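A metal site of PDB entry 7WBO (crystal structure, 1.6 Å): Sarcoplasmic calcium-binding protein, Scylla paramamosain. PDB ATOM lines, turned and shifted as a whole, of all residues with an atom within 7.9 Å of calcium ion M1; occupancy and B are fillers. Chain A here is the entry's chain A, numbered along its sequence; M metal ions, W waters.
The backbone NH of Gly 120 lies close to the side-chain carboxylate of Asp 117 (3.3 Å).
The side-chain carboxylate of Asp 117 lies within hydrogen-bond range of the backbone NH of Gly 122.
The backbone NH (N) of Gly 125 lies close to the side-chain carboxylate (OE1) of Glu 128 (3.2 Å).
The backbone NH of Ile 118 lies close to the side-chain carboxylate of Glu 128 (3.2 Å).
Within 4 Å of calcium ion M1: Asp 117, Asn 119, Asp 121, Leu 123 and Glu 128.
Calcium ion M1 is bound by the side-chain carboxylate (OD1) of Asp 117 (2.3 Å), the backbone carbonyl oxygen (O) of Leu 123 (2.3 Å), the side-chain amide oxygen (OD1) of Asn 119 (2.4 Å), the side-chain carboxylate (OD1) of Asp 121 (2.4 Å), the side-chain carboxylate (OE1) of Glu 128 (2.4 Å), water W1 (2.4 Å) and the side-chain carboxylate (OE2) of Glu 128 (2.5 Å).
Water W1 bridges the side-chain amide nitrogen of Asn 119 (3.2 Å) and the side-chain carboxylate of Asp 121 (3.5 Å).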
ATOM      1  N   PHE A 113       1.799  16.482  21.854  1.00  0.00           N
ATOM      2  CA  PHE A 113       1.752  17.106  20.512  1.00  0.00           C
ATOM      3  C   PHE A 113       2.798  18.208  20.394  1.00  0.00           C
ATOM      4  O   PHE A 113       3.466  18.281  19.368  1.00  0.00           O
ATOM      5  CB  PHE A 113       0.344  17.639  20.243  1.00  0.00           C
ATOM      6  CG  PHE A 113       0.172  18.269  18.877  1.00  0.00           C
ATOM      7  CD1 PHE A 113       0.439  19.608  18.634  1.00  0.00           C
ATOM      8  CD2 PHE A 113      -0.309  17.483  17.859  1.00  0.00           C
ATOM      9  CE1 PHE A 113       0.336  20.114  17.349  1.00  0.00           C
ATOM     10  CE2 PHE A 113      -0.496  18.018  16.600  1.00  0.00           C
ATOM     11  CZ  PHE A 113      -0.199  19.312  16.347  1.00  0.00           C
ATOM     12  N   ILE A 116       6.200  16.657  19.859  1.00  0.00           N
ATOM     13  CA  ILE A 116       6.366  16.036  18.525  1.00  0.00           C
ATOM     14  C   ILE A 116       6.527  17.135  17.480  1.00  0.00           C
ATOM     15  O   ILE A 116       7.208  16.895  16.456  1.00  0.00           O
ATOM     16  CB  ILE A 116       5.165  15.116  18.217  1.00  0.00           C
ATOM     17  CG1 ILE A 116       5.124  13.939  19.195  1.00  0.00           C
ATOM     18  CG2 ILE A 116       5.216  14.606  16.773  1.00  0.00           C
ATOM     19  CD1 ILE A 116       3.874  13.065  19.020  1.00  0.00           C
ATOM     20  N   ASP A 117       5.793  18.226  17.650  1.00  0.00           N
ATOM     21  CA  ASP A 117       5.762  19.300  16.629  1.00  0.00           C
ATOM     22  C   ASP A 117       7.041  20.136  16.759  1.00  0.00           C
ATOM     23  O   ASP A 117       6.932  21.318  17.193  1.00  0.00           O
ATOM     24  CB  ASP A 117       4.539  20.164  16.827  1.00  0.00           C
ATOM     25  CG  ASP A 117       4.397  21.309  15.863  1.00  0.00           C
ATOM     26  OD1 ASP A 117       4.977  21.230  14.750  1.00  0.00           O
ATOM     27  OD2 ASP A 117       3.646  22.267  16.231  1.00  0.00           O
ATOM     28  N   ILE A 118       8.160  19.549  16.328  1.00  0.00           N
ATOM     29  CA  ILE A 118       9.508  20.141  16.543  1.00  0.00           C
ATOM     30  C   ILE A 118       9.565  21.515  15.898  1.00  0.00           C
ATOM     31  O   ILE A 118      10.170  22.433  16.513  1.00  0.00           O
ATOM     32  CB  ILE A 118      10.615  19.205  16.023  1.00  0.00           C
ATOM     33  CG1 ILE A 118      10.667  17.917  16.842  1.00  0.00           C
ATOM     34  CG2 ILE A 118      11.942  19.938  16.065  1.00  0.00           C
ATOM     35  CD1 ILE A 118      11.241  16.759  16.083  1.00  0.00           C
ATOM     36  N   ASN A 119       8.971  21.721  14.725  1.00  0.00           N
ATOM     37  CA  ASN A 119       9.152  23.029  14.040  1.00  0.00           C
ATOM     38  C   ASN A 119       8.088  24.025  14.517  1.00  0.00           C
ATOM     39  O   ASN A 119       8.108  25.159  14.040  1.00  0.00           O
ATOM     40  CB  ASN A 119       9.242  22.860  12.529  1.00  0.00           C
ATOM     41  CG  ASN A 119       7.965  22.406  11.875  1.00  0.00           C
ATOM     42  OD1 ASN A 119       6.915  22.296  12.527  1.00  0.00           O
ATOM     43  ND2 ASN A 119       8.063  22.025  10.622  1.00  0.00           N
ATOM     44  N   GLY A 120       7.149  23.623  15.396  1.00  0.00           N
ATOM     45  CA  GLY A 120       6.192  24.541  16.026  1.00  0.00           C
ATOM     46  C   GLY A 120       5.171  25.112  15.070  1.00  0.00           C
ATOM     47  O   GLY A 120       4.566  26.164  15.418  1.00  0.00           O
ATOM     48  N   ASP A 121       4.917  24.487  13.924  1.00  0.00           N
ATOM     49  CA  ASP A 121       3.950  25.005  12.924  1.00  0.00           C
ATOM     50  C   ASP A 121       2.513  24.508  13.212  1.00  0.00           C
ATOM     51  O   ASP A 121       1.630  24.834  12.426  1.00  0.00           O
ATOM     52  CB  ASP A 121       4.368  24.714  11.500  1.00  0.00           C
ATOM     53  CG  ASP A 121       4.274  23.272  11.032  1.00  0.00           C
ATOM     54  OD1 ASP A 121       4.072  22.393  11.899  1.00  0.00           O
ATOM     55  OD2 ASP A 121       4.371  23.032   9.821  1.00  0.00           O
ATOM     56  N   GLY A 122       2.300  23.799  14.309  1.00  0.00           N
ATOM     57  CA  GLY A 122       0.948  23.363  14.677  1.00  0.00           C
ATOM     58  C   GLY A 122       0.462  22.151  13.905  1.00  0.00           C
ATOM     59  O   GLY A 122      -0.727  21.796  14.004  1.00  0.00           O
ATOM     60  N   LEU A 123       1.335  21.512  13.158  1.00  0.00           N
ATOM     61  CA  LEU A 123       0.993  20.290  12.408  1.00  0.00           C
ATOM     62  C   LEU A 123       2.075  19.240  12.681  1.00  0.00           C
ATOM     63  O   LEU A 123       3.290  19.599  12.630  1.00  0.00           O
ATOM     64  CB  LEU A 123       0.966  20.590  10.918  1.00  0.00           C
ATOM     65  CG  LEU A 123      -0.111  21.557  10.459  1.00  0.00           C
ATOM     66  CD1 LEU A 123       0.166  22.056   9.041  1.00  0.00           C
ATOM     67  CD2 LEU A 123      -1.485  20.926  10.548  1.00  0.00           C
ATOM     68  N   VAL A 124       1.681  18.012  12.936  1.00  0.00           N
ATOM     69  CA  VAL A 124       2.673  16.905  12.932  1.00  0.00           C
ATOM     70  C   VAL A 124       2.765  16.392  11.502  1.00  0.00           C
ATOM     71  O   VAL A 124       1.815  15.747  11.006  1.00  0.00           O
ATOM     72  CB  VAL A 124       2.288  15.823  13.957  1.00  0.00           C
ATOM     73  CG1 VAL A 124       3.132  14.550  13.806  1.00  0.00           C
ATOM     74  CG2 VAL A 124       2.407  16.397  15.377  1.00  0.00           C
ATOM     75  N   GLY A 125       3.859  16.682  10.825  1.00  0.00           N
ATOM     76  CA  GLY A 125       4.113  16.164   9.488  1.00  0.00           C
ATOM     77  C   GLY A 125       4.878  14.845   9.523  1.00  0.00           C
ATOM     78  O   GLY A 125       5.127  14.285  10.606  1.00  0.00           O
ATOM     79  N   VAL A 126       5.140  14.301   8.359  1.00  0.00           N
ATOM     80  CA  VAL A 126       5.751  12.951   8.248  1.00  0.00           C
ATOM     81  C   VAL A 126       7.123  12.874   8.932  1.00  0.00           C
ATOM     82  O   VAL A 126       7.386  11.891   9.613  1.00  0.00           O
ATOM     83  CB  VAL A 126       5.814  12.451   6.808  1.00  0.00           C
ATOM     84  CG1 VAL A 126       6.808  13.216   5.972  1.00  0.00           C
ATOM     85  CG2 VAL A 126       6.040  10.972   6.820  1.00  0.00           C
ATOM     86  N   GLU A 128       8.242  14.602  11.500  1.00  0.00           N
ATOM     87  CA  GLU A 128       8.008  14.626  12.964  1.00  0.00           C
ATOM     88  C   GLU A 128       7.435  13.285  13.406  1.00  0.00           C
ATOM     89  O   GLU A 128       7.794  12.759  14.466  1.00  0.00           O
ATOM     90  CB  GLU A 128       7.147  15.802  13.343  1.00  0.00           C
ATOM     91  CG  GLU A 128       7.855  17.112  13.128  1.00  0.00           C
ATOM     92  CD  GLU A 128       6.988  18.356  13.098  1.00  0.00           C
ATOM     93  OE1 GLU A 128       5.739  18.205  12.974  1.00  0.00           O
ATOM     94  OE2 GLU A 128       7.554  19.464  13.165  1.00  0.00           O
ATOM     95  N   GLY A 161      -0.844  19.402   5.249  1.00  0.00           N
ATOM     96  CA  GLY A 161       0.591  19.147   5.479  1.00  0.00           C
ATOM     97  C   GLY A 161       0.831  18.474   6.806  1.00  0.00           C
ATOM     98  O   GLY A 161       2.026  18.430   7.247  1.00  0.00           O
ATOM     99  N   GLY A 162      -0.204  17.940   7.438  1.00  0.00           N
ATOM    100  CA  GLY A 162       0.030  17.159   8.644  1.00  0.00           C
ATOM    101  C   GLY A 162      -1.177  17.205   9.548  1.00  0.00           C
ATOM    102  O   GLY A 162      -2.247  17.638   9.168  1.00  0.00           O
ATOM    103  N   ILE A 163      -0.970  16.723  10.760  1.00  0.00           N
ATOM    104  CA  ILE A 163      -2.042  16.502  11.734  1.00  0.00           C
ATOM    105  C   ILE A 163      -2.071  17.664  12.696  1.00  0.00           C
ATOM    106  O   ILE A 163      -1.077  17.932  13.367  1.00  0.00           O
ATOM    107  CB  ILE A 163      -1.823  15.186  12.522  1.00  0.00           C
ATOM    108  CG1 ILE A 163      -1.682  13.964  11.607  1.00  0.00           C
ATOM    109  CG2 ILE A 163      -2.973  15.027  13.496  1.00  0.00           C
ATOM    110  CD1 ILE A 163      -1.252  12.714  12.243  1.00  0.00           C
HETATM  111 CA    CA M   1       5.341  20.545  12.630  1.00  0.00          CA
HETATM  112 CA    CA M   2       7.317  17.273   9.669  1.00  0.00          CA
HETATM  113  O   HOH W   1       5.745  19.875  10.332  1.00  0.00           O
